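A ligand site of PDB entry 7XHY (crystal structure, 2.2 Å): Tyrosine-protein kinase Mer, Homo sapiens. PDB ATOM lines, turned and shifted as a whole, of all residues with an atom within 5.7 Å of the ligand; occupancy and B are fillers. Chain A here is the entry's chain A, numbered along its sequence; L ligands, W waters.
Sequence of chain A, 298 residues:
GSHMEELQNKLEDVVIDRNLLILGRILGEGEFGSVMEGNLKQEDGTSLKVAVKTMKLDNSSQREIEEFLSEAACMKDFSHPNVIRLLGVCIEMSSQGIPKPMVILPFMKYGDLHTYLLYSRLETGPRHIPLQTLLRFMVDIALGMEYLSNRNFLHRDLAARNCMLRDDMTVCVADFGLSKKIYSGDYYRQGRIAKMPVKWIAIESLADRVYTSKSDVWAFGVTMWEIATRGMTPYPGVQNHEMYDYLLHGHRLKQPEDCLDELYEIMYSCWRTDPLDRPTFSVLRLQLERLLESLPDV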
ATOM      1  N   LEU A  27       3.878 -21.025   0.114  1.00  0.00           N
ATOM      2  CA  LEU A  27       3.933 -22.439  -0.189  1.00  0.00           C
ATOM      3  C   LEU A  27       2.530 -23.061  -0.198  1.00  0.00           C
ATOM      4  O   LEU A  27       2.322 -24.056  -0.898  1.00  0.00           O
ATOM      5  CB  LEU A  27       4.818 -23.151   0.841  1.00  0.00           C
ATOM      6  CG  LEU A  27       6.226 -22.580   0.983  1.00  0.00           C
ATOM      7  CD1 LEU A  27       6.956 -23.187   2.173  1.00  0.00           C
ATOM      8  CD2 LEU A  27       7.003 -22.806  -0.289  1.00  0.00           C
ATOM      9  N   VAL A  35       1.069 -20.932   4.651  1.00  0.00           N
ATOM     10  CA  VAL A  35       2.446 -21.327   4.928  1.00  0.00           C
ATOM     11  C   VAL A  35       3.353 -20.635   3.924  1.00  0.00           C
ATOM     12  O   VAL A  35       3.135 -20.726   2.716  1.00  0.00           O
ATOM     13  CB  VAL A  35       2.654 -22.848   4.876  1.00  0.00           C
ATOM     14  CG1 VAL A  35       4.109 -23.179   5.199  1.00  0.00           C
ATOM     15  CG2 VAL A  35       1.709 -23.536   5.820  1.00  0.00           C
ATOM     16  N   ALA A  51      10.138 -22.393   7.548  1.00  0.00           N
ATOM     17  CA  ALA A  51       8.746 -22.267   7.145  1.00  0.00           C
ATOM     18  C   ALA A  51       7.982 -21.452   8.177  1.00  0.00           C
ATOM     19  O   ALA A  51       8.245 -21.556   9.377  1.00  0.00           O
ATOM     20  CB  ALA A  51       8.109 -23.641   6.979  1.00  0.00           C
ATOM     21  N   VAL A  52       7.067 -20.605   7.710  1.00  0.00           N
ATOM     22  CA  VAL A  52       6.322 -19.700   8.563  1.00  0.00           C
ATOM     23  C   VAL A  52       4.834 -19.962   8.348  1.00  0.00           C
ATOM     24  O   VAL A  52       4.359 -19.916   7.200  1.00  0.00           O
ATOM     25  CB  VAL A  52       6.661 -18.230   8.290  1.00  0.00           C
ATOM     26  CG1 VAL A  52       6.069 -17.343   9.351  1.00  0.00           C
ATOM     27  CG2 VAL A  52       8.181 -18.044   8.215  1.00  0.00           C
ATOM     28  N   LYS A  53       4.102 -20.233   9.424  1.00  0.00           N
ATOM     29  CA  LYS A  53       2.664 -20.477   9.341  1.00  0.00           C
ATOM     30  C   LYS A  53       1.916 -19.328  10.006  1.00  0.00           C
ATOM     31  O   LYS A  53       2.177 -19.008  11.161  1.00  0.00           O
ATOM     32  CB  LYS A  53       2.289 -21.816   9.968  1.00  0.00           C
ATOM     33  CG  LYS A  53       0.836 -22.219   9.693  1.00  0.00           C
ATOM     34  CD  LYS A  53       0.393 -23.337  10.591  1.00  0.00           C
ATOM     35  CE  LYS A  53       0.013 -22.824  11.963  1.00  0.00           C
ATOM     36  NZ  LYS A  53       0.017 -23.928  12.947  1.00  0.00           N
ATOM     37  N   ALA A  72       2.404 -23.263  21.889  1.00  0.00           N
ATOM     38  CA  ALA A  72       3.646 -23.174  21.135  1.00  0.00           C
ATOM     39  C   ALA A  72       4.857 -23.348  22.047  1.00  0.00           C
ATOM     40  O   ALA A  72       5.778 -24.104  21.726  1.00  0.00           O
ATOM     41  CB  ALA A  72       3.706 -21.843  20.388  1.00  0.00           C
ATOM     42  N   MET A  75       5.298 -27.011  22.861  1.00  0.00           N
ATOM     43  CA  MET A  75       5.839 -27.818  21.766  1.00  0.00           C
ATOM     44  C   MET A  75       7.317 -27.541  21.551  1.00  0.00           C
ATOM     45  O   MET A  75       8.104 -28.477  21.342  1.00  0.00           O
ATOM     46  CB  MET A  75       5.054 -27.553  20.473  1.00  0.00           C
ATOM     47  CG  MET A  75       5.481 -28.414  19.263  1.00  0.00           C
ATOM     48  SD  MET A  75       5.757 -30.184  19.660  1.00  0.00           S
ATOM     49  CE  MET A  75       4.088 -30.692  20.088  1.00  0.00           C
ATOM     50  N   VAL A  83      10.000 -35.597  16.352  1.00  0.00           N
ATOM     51  CA  VAL A  83       8.972 -34.615  16.608  1.00  0.00           C
ATOM     52  C   VAL A  83       9.476 -33.322  15.998  1.00  0.00           C
ATOM     53  O   VAL A  83      10.627 -32.942  16.251  1.00  0.00           O
ATOM     54  CB  VAL A  83       8.708 -34.432  18.116  1.00  0.00           C
ATOM     55  CG1 VAL A  83       7.716 -33.319  18.334  1.00  0.00           C
ATOM     56  CG2 VAL A  83       8.270 -35.769  18.735  1.00  0.00           C
ATOM     57  N   ILE A  84       8.647 -32.652  15.195  1.00  0.00           N
ATOM     58  CA  ILE A  84       9.120 -31.457  14.516  1.00  0.00           C
ATOM     59  C   ILE A  84       9.548 -30.412  15.539  1.00  0.00           C
ATOM     60  O   ILE A  84       8.893 -30.205  16.577  1.00  0.00           O
ATOM     61  CB  ILE A  84       8.050 -30.902  13.567  1.00  0.00           C
ATOM     62  CG1 ILE A  84       8.685 -29.848  12.663  1.00  0.00           C
ATOM     63  CG2 ILE A  84       6.871 -30.355  14.380  1.00  0.00           C
ATOM     64  CD1 ILE A  84       7.843 -29.500  11.521  1.00  0.00           C
ATOM     65  N   LEU A  86       9.833 -26.839  16.864  1.00  0.00           N
ATOM     66  CA  LEU A  86       9.187 -25.545  16.715  1.00  0.00           C
ATOM     67  C   LEU A  86      10.177 -24.471  17.150  1.00  0.00           C
ATOM     68  O   LEU A  86      10.515 -24.359  18.330  1.00  0.00           O
ATOM     69  CB  LEU A  86       7.909 -25.499  17.538  1.00  0.00           C
ATOM     70  CG  LEU A  86       6.830 -24.435  17.280  1.00  0.00           C
ATOM     71  CD1 LEU A  86       5.494 -24.960  17.725  1.00  0.00           C
ATOM     72  CD2 LEU A  86       7.120 -23.143  18.016  1.00  0.00           C
ATOM     73  N   VAL A 103       4.071 -19.118  13.336  1.00  0.00           N
ATOM     74  CA  VAL A 103       4.889 -20.207  13.874  1.00  0.00           C
ATOM     75  C   VAL A 103       6.065 -20.434  12.926  1.00  0.00           C
ATOM     76  O   VAL A 103       5.867 -20.547  11.710  1.00  0.00           O
ATOM     77  CB  VAL A 103       4.076 -21.504  14.023  1.00  0.00           C
ATOM     78  CG1 VAL A 103       4.915 -22.583  14.685  1.00  0.00           C
ATOM     79  CG2 VAL A 103       2.796 -21.240  14.792  1.00  0.00           C
ATOM     80  N   LEU A 105       9.255 -22.885  11.835  1.00  0.00           N
ATOM     81  CA  LEU A 105       9.782 -24.241  11.841  1.00  0.00           C
ATOM     82  C   LEU A 105      10.913 -24.310  10.822  1.00  0.00           C
ATOM     83  O   LEU A 105      11.017 -23.451   9.951  1.00  0.00           O
ATOM     84  CB  LEU A 105       8.691 -25.269  11.485  1.00  0.00           C
ATOM     85  CG  LEU A 105       7.440 -25.063  12.353  1.00  0.00           C
ATOM     86  CD1 LEU A 105       6.451 -24.223  11.607  1.00  0.00           C
ATOM     87  CD2 LEU A 105       6.839 -26.364  12.806  1.00  0.00           C
ATOM     88  N   PRO A 106      11.783 -25.321  10.906  1.00  0.00           N
ATOM     89  CA  PRO A 106      12.783 -25.488   9.838  1.00  0.00           C
ATOM     90  C   PRO A 106      12.128 -25.805   8.500  1.00  0.00           C
ATOM     91  O   PRO A 106      11.161 -26.569   8.422  1.00  0.00           O
ATOM     92  CB  PRO A 106      13.637 -26.652  10.330  1.00  0.00           C
ATOM     93  CG  PRO A 106      13.340 -26.780  11.801  1.00  0.00           C
ATOM     94  CD  PRO A 106      11.926 -26.307  11.975  1.00  0.00           C
ATOM     95  N   PHE A 107      12.635 -25.190   7.429  1.00  0.00           N
ATOM     96  CA  PHE A 107      12.123 -25.509   6.099  1.00  0.00           C
ATOM     97  C   PHE A 107      12.572 -26.913   5.710  1.00  0.00           C
ATOM     98  O   PHE A 107      13.762 -27.229   5.761  1.00  0.00           O
ATOM     99  CB  PHE A 107      12.584 -24.485   5.060  1.00  0.00           C
ATOM    100  CG  PHE A 107      12.094 -24.785   3.663  1.00  0.00           C
ATOM    101  CD1 PHE A 107      10.777 -24.508   3.297  1.00  0.00           C
ATOM    102  CD2 PHE A 107      12.944 -25.346   2.714  1.00  0.00           C
ATOM    103  CE1 PHE A 107      10.326 -24.778   2.014  1.00  0.00           C
ATOM    104  CE2 PHE A 107      12.506 -25.618   1.432  1.00  0.00           C
ATOM    105  CZ  PHE A 107      11.189 -25.346   1.075  1.00  0.00           C
ATOM    106  N   MET A 108      11.618 -27.748   5.319  1.00  0.00           N
ATOM    107  CA  MET A 108      11.877 -29.114   4.866  1.00  0.00           C
ATOM    108  C   MET A 108      11.437 -29.241   3.398  1.00  0.00           C
ATOM    109  O   MET A 108      10.238 -29.321   3.096  1.00  0.00           O
ATOM    110  CB  MET A 108      11.192 -30.106   5.785  1.00  0.00           C
ATOM    111  CG  MET A 108      11.827 -30.109   7.176  1.00  0.00           C
ATOM    112  SD  MET A 108      10.926 -31.151   8.323  1.00  0.00           S
ATOM    113  CE  MET A 108       9.435 -30.171   8.257  1.00  0.00           C
ATOM    114  N   LYS A 109      12.435 -29.272   2.508  1.00  0.00           N
ATOM    115  CA  LYS A 109      12.193 -29.249   1.072  1.00  0.00           C
ATOM    116  C   LYS A 109      11.485 -30.490   0.565  1.00  0.00           C
ATOM    117  O   LYS A 109      10.949 -30.447  -0.537  1.00  0.00           O
ATOM    118  CB  LYS A 109      13.510 -29.077   0.316  1.00  0.00           C
ATOM    119  CG  LYS A 109      14.493 -30.214   0.475  1.00  0.00           C
ATOM    120  CD  LYS A 109      15.613 -30.045  -0.530  1.00  0.00           C
ATOM    121  CE  LYS A 109      16.849 -30.895  -0.247  1.00  0.00           C
ATOM    122  NZ  LYS A 109      17.916 -30.556  -1.270  1.00  0.00           N
ATOM    123  N   GLY A 111       8.805 -31.680   2.056  1.00  0.00           N
ATOM    124  CA  GLY A 111       7.398 -31.506   2.355  1.00  0.00           C
ATOM    125  C   GLY A 111       6.830 -32.595   3.250  1.00  0.00           C
ATOM    126  O   GLY A 111       7.560 -33.301   3.962  1.00  0.00           O
ATOM    127  N   MET A 145       5.797 -40.452  18.409  1.00  0.00           N
ATOM    128  CA  MET A 145       4.563 -40.635  19.170  1.00  0.00           C
ATOM    129  C   MET A 145       4.814 -41.322  20.499  1.00  0.00           C
ATOM    130  O   MET A 145       4.100 -41.055  21.469  1.00  0.00           O
ATOM    131  CB  MET A 145       3.557 -41.455  18.355  1.00  0.00           C
ATOM    132  CG  MET A 145       2.855 -40.709  17.233  1.00  0.00           C
ATOM    133  SD  MET A 145       2.159 -39.122  17.731  1.00  0.00           S
ATOM    134  CE  MET A 145       0.689 -39.629  18.660  1.00  0.00           C
ATOM    135  N   LEU A 148       5.999 -38.508  22.658  1.00  0.00           N
ATOM    136  CA  LEU A 148       4.913 -37.596  22.993  1.00  0.00           C
ATOM    137  C   LEU A 148       3.964 -38.222  24.016  1.00  0.00           C
ATOM    138  O   LEU A 148       3.567 -37.578  24.997  1.00  0.00           O
ATOM    139  CB  LEU A 148       4.144 -37.202  21.727  1.00  0.00           C
ATOM    140  CG  LEU A 148       4.865 -36.307  20.714  1.00  0.00           C
ATOM    141  CD1 LEU A 148       4.025 -36.127  19.435  1.00  0.00           C
ATOM    142  CD2 LEU A 148       5.216 -34.955  21.331  1.00  0.00           C
ATOM    143  N   PHE A 153       1.024 -36.129  26.109  1.00  0.00           N
ATOM    144  CA  PHE A 153       0.606 -35.289  25.000  1.00  0.00           C
ATOM    145  C   PHE A 153      -0.311 -36.085  24.085  1.00  0.00           C
ATOM    146  O   PHE A 153       0.010 -37.224  23.695  1.00  0.00           O
ATOM    147  CB  PHE A 153       1.830 -34.763  24.240  1.00  0.00           C
ATOM    148  CG  PHE A 153       1.484 -33.732  23.200  1.00  0.00           C
ATOM    149  CD1 PHE A 153       1.358 -32.398  23.541  1.00  0.00           C
ATOM    150  CD2 PHE A 153       1.224 -34.120  21.904  1.00  0.00           C
ATOM    151  CE1 PHE A 153       1.004 -31.472  22.603  1.00  0.00           C
ATOM    152  CE2 PHE A 153       0.882 -33.175  20.944  1.00  0.00           C
ATOM    153  CZ  PHE A 153       0.775 -31.855  21.292  1.00  0.00           C
ATOM    154  N   HIS A 155      -2.095 -36.075  20.413  1.00  0.00           N
ATOM    155  CA  HIS A 155      -1.951 -35.413  19.118  1.00  0.00           C
ATOM    156  C   HIS A 155      -3.296 -34.968  18.587  1.00  0.00           C
ATOM    157  O   HIS A 155      -3.505 -33.795  18.287  1.00  0.00           O
ATOM    158  CB  HIS A 155      -1.262 -36.337  18.120  1.00  0.00           C
ATOM    159  CG  HIS A 155      -0.850 -35.629  16.856  1.00  0.00           C
ATOM    160  ND1 HIS A 155      -1.748 -35.011  16.025  1.00  0.00           N
ATOM    161  CD2 HIS A 155       0.360 -35.462  16.288  1.00  0.00           C
ATOM    162  CE1 HIS A 155      -1.112 -34.481  14.996  1.00  0.00           C
ATOM    163  NE2 HIS A 155       0.173 -34.744  15.124  1.00  0.00           N
ATOM    164  N   MET A 164       6.254 -34.861   8.488  1.00  0.00           N
ATOM    165  CA  MET A 164       7.154 -34.093   7.628  1.00  0.00           C
ATOM    166  C   MET A 164       8.438 -34.872   7.371  1.00  0.00           C
ATOM    167  O   MET A 164       8.899 -35.641   8.227  1.00  0.00           O
ATOM    168  CB  MET A 164       7.454 -32.732   8.254  1.00  0.00           C
ATOM    169  CG  MET A 164       6.250 -31.795   8.402  1.00  0.00           C
ATOM    170  SD  MET A 164       5.478 -31.329   6.818  1.00  0.00           S
ATOM    171  CE  MET A 164       6.776 -30.419   5.968  1.00  0.00           C
ATOM    172  N   VAL A 173       6.936 -35.955  13.518  1.00  0.00           N
ATOM    173  CA  VAL A 173       5.509 -35.725  13.707  1.00  0.00           C
ATOM    174  C   VAL A 173       5.270 -34.242  13.917  1.00  0.00           C
ATOM    175  O   VAL A 173       5.996 -33.571  14.655  1.00  0.00           O
ATOM    176  CB  VAL A 173       4.993 -36.550  14.892  1.00  0.00           C
ATOM    177  CG1 VAL A 173       3.494 -36.330  15.053  1.00  0.00           C
ATOM    178  CG2 VAL A 173       5.313 -38.016  14.680  1.00  0.00           C
ATOM    179  N   ALA A 174       4.212 -33.737  13.288  1.00  0.00           N
ATOM    180  CA  ALA A 174       3.872 -32.326  13.283  1.00  0.00           C
ATOM    181  C   ALA A 174       2.360 -32.188  13.271  1.00  0.00           C
ATOM    182  O   ALA A 174       1.628 -33.172  13.384  1.00  0.00           O
ATOM    183  CB  ALA A 174       4.514 -31.641  12.064  1.00  0.00           C
ATOM    184  N   ASP A 175       1.868 -30.957  13.134  1.00  0.00           N
ATOM    185  CA  ASP A 175       0.431 -30.721  12.980  1.00  0.00           C
ATOM    186  C   ASP A 175       0.238 -29.368  12.310  1.00  0.00           C
ATOM    187  O   ASP A 175       0.451 -28.328  12.944  1.00  0.00           O
ATOM    188  CB  ASP A 175      -0.257 -30.786  14.335  1.00  0.00           C
ATOM    189  CG  ASP A 175      -1.755 -30.642  14.237  1.00  0.00           C
ATOM    190  OD1 ASP A 175      -2.271 -30.355  13.133  1.00  0.00           O
ATOM    191  OD2 ASP A 175      -2.417 -30.838  15.284  1.00  0.00           O
ATOM    192  N   PHE A 176      -0.164 -29.374  11.041  1.00  0.00           N
ATOM    193  CA  PHE A 176      -0.381 -28.100  10.371  1.00  0.00           C
ATOM    194  C   PHE A 176      -1.432 -27.254  11.078  1.00  0.00           C
ATOM    195  O   PHE A 176      -1.442 -26.026  10.907  1.00  0.00           O
ATOM    196  CB  PHE A 176      -0.815 -28.326   8.920  1.00  0.00           C
ATOM    197  CG  PHE A 176       0.337 -28.573   7.968  1.00  0.00           C
ATOM    198  CD1 PHE A 176       0.878 -29.846   7.837  1.00  0.00           C
ATOM    199  CD2 PHE A 176       0.847 -27.536   7.174  1.00  0.00           C
ATOM    200  CE1 PHE A 176       1.913 -30.089   6.928  1.00  0.00           C
ATOM    201  CE2 PHE A 176       1.869 -27.765   6.271  1.00  0.00           C
ATOM    202  CZ  PHE A 176       2.401 -29.048   6.145  1.00  0.00           C
HETATM  203  C1  LIG L   1       4.475 -26.729   8.235  1.00  0.00           C
HETATM  204  C2  LIG L   1       4.451 -27.984   8.811  1.00  0.00           C
HETATM  205  C3  LIG L   1       4.137 -28.100  10.148  1.00  0.00           C
HETATM  206  C4  LIG L   1       3.830 -26.983  10.895  1.00  0.00           C
HETATM  207  C5  LIG L   1       3.822 -25.749  10.303  1.00  0.00           C
HETATM  208  C6  LIG L   1       4.147 -25.610   8.968  1.00  0.00           C
HETATM  209  C7  LIG L   1       2.996 -26.189  13.225  1.00  0.00           C
HETATM  210  C8  LIG L   1       2.675 -26.686  14.618  1.00  0.00           C
HETATM  211  C9  LIG L   1       2.133 -25.819  15.562  1.00  0.00           C
HETATM  212  C10 LIG L   1       1.997 -27.576  17.111  1.00  0.00           C
HETATM  213  C11 LIG L   1       2.518 -28.446  16.162  1.00  0.00           C
HETATM  214  C12 LIG L   1       2.850 -28.000  14.916  1.00  0.00           C
HETATM  215  C13 LIG L   1       2.694 -29.901  16.567  1.00  0.00           C
HETATM  216  C14 LIG L   1       3.921 -30.533  16.508  1.00  0.00           C
HETATM  217  C15 LIG L   1       4.054 -31.858  16.874  1.00  0.00           C
HETATM  218  C16 LIG L   1       2.904 -32.534  17.310  1.00  0.00           C
HETATM  219  C17 LIG L   1       1.668 -31.917  17.382  1.00  0.00           C
HETATM  220  C18 LIG L   1       7.737 -27.175   4.859  1.00  0.00           C
HETATM  221  C19 LIG L   1       6.431 -26.940   5.263  1.00  0.00           C
HETATM  222  C20 LIG L   1       6.130 -26.821   6.570  1.00  0.00           C
HETATM  223  C21 LIG L   1       7.115 -26.920   7.490  1.00  0.00           C
HETATM  224  C22 LIG L   1       8.419 -27.172   7.087  1.00  0.00           C
HETATM  225  C23 LIG L   1       1.565 -30.587  17.001  1.00  0.00           C
HETATM  226  F1  LIG L   1       3.006 -33.818  17.682  1.00  0.00           F
HETATM  227  F2  LIG L   1       4.145 -24.388   8.382  1.00  0.00           F
HETATM  228  N1  LIG L   1       8.719 -27.304   5.774  1.00  0.00           N
HETATM  229  N2  LIG L   1       8.062 -27.324   3.470  1.00  0.00           N
HETATM  230  N3  LIG L   1       3.492 -27.184  12.286  1.00  0.00           N
HETATM  231  N4  LIG L   1       1.807 -26.279  16.790  1.00  0.00           N
HETATM  232  O1  LIG L   1       4.789 -26.567   6.888  1.00  0.00           O
HETATM  233  O2  LIG L   1       3.299 -28.751  14.102  1.00  0.00           O
HETATM  234  O3  LIG L   1       2.763 -25.083  12.932  1.00  0.00           O
HETATM  235 CL1  LIG L   1       5.079 -26.780   4.081  1.00  0.00          CL
HETATM  236  O   HOH W   1      -1.715 -31.760  17.447  1.00  0.00           O
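An oxygen (O3) of the ligand lies within hydrogen-bond range of the side-chain amino group of Lys 53, at 3.0 Å.
N of Asp 175 is in hydrogen-bond range of O2 of the ligand, at 2.8 Å.
The backbone carbonyl oxygen (O) of Asp 175 sits close to a nitrogen (N3) of the ligand (3.3 Å).
A nitrogen (N1) of the ligand lies within hydrogen-bond range of the backbone NH (N) of Met 108.
A nitrogen (N2) of the ligand lies within hydrogen-bond range of the backbone carbonyl oxygen of Met 108, at 3.0 Å.
The backbone NH of Val 103 is in hydrogen-bond range of the backbone carbonyl oxygen of Lys 53.
O of Val 173 lies within hydrogen-bond range of N of Ile 84.
The backbone NH (N) of Phe 153 sits at hydrogen-bond distance from the backbone carbonyl oxygen (O) of Leu 148.
The backbone carbonyl oxygen (O) of Phe 176 sits at hydrogen-bond distance from the side-chain amino group (NZ) of Lys 53, 3.3 Å away.
O of Ala 174 is in hydrogen-bond range of NE2 of His 155 (2.8 Å).
The backbone carbonyl oxygen of Leu 105 is in hydrogen-bond range of the backbone NH of Ala 51 (2.8 Å).
O of Val 35 is in hydrogen-bond range of N of Leu 27.
Val 35 touches the ligand.
Ala 51 touches the ligand (CB to C21, 3.5 Å).
Met 75 touches the ligand.
Ile 84 touches the ligand.
Val 103 touches the ligand.
CD1 of Leu 105 touches C5 of the ligand, at 3.3 Å.
O of Pro 106 touches C22 of the ligand (3.1 Å).
Phe 107 touches the ligand (CE1 to N2, 3.7 Å).
Leu 148 touches the ligand.
CE2 of Phe 153 touches C17 of the ligand, at 3.9 Å.
His 155 touches the ligand (CD2 to F1, 3.4 Å).
CE of Met 164 touches C18 of the ligand (3.6 Å).
Val 173 touches the ligand.
Ala 174 touches the ligand (CA to C15, 3.6 Å).
CE2 of Phe 176 touches O1 of the ligand, at 3.2 Å.
Hydrophobic or aromatic side chains that line the ligand: Val 35, Ala 51, Met 75, Ile 84, Val 103, Leu 105, Phe 107, Met 108, Leu 148, Phe 153, His 155, Met 164, Val 173, Ala 174 and Phe 176.
Within 4 Å of the ligand: Val 35, Ala 51, Lys 53, Met 75, Ile 84, Val 103, Leu 105, Pro 106, Phe 107, Met 108, Leu 148, Phe 153, His 155, Met 164, Val 173, Ala 174, Asp 175 and Phe 176.
The nearest printed residue that does not touch the ligand is Leu 86 (4.03 Å).
Water W1 lies within hydrogen-bond range of the side-chain carboxylate (OD2) of Asp 175 and the backbone carbonyl oxygen (O) of His 155.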
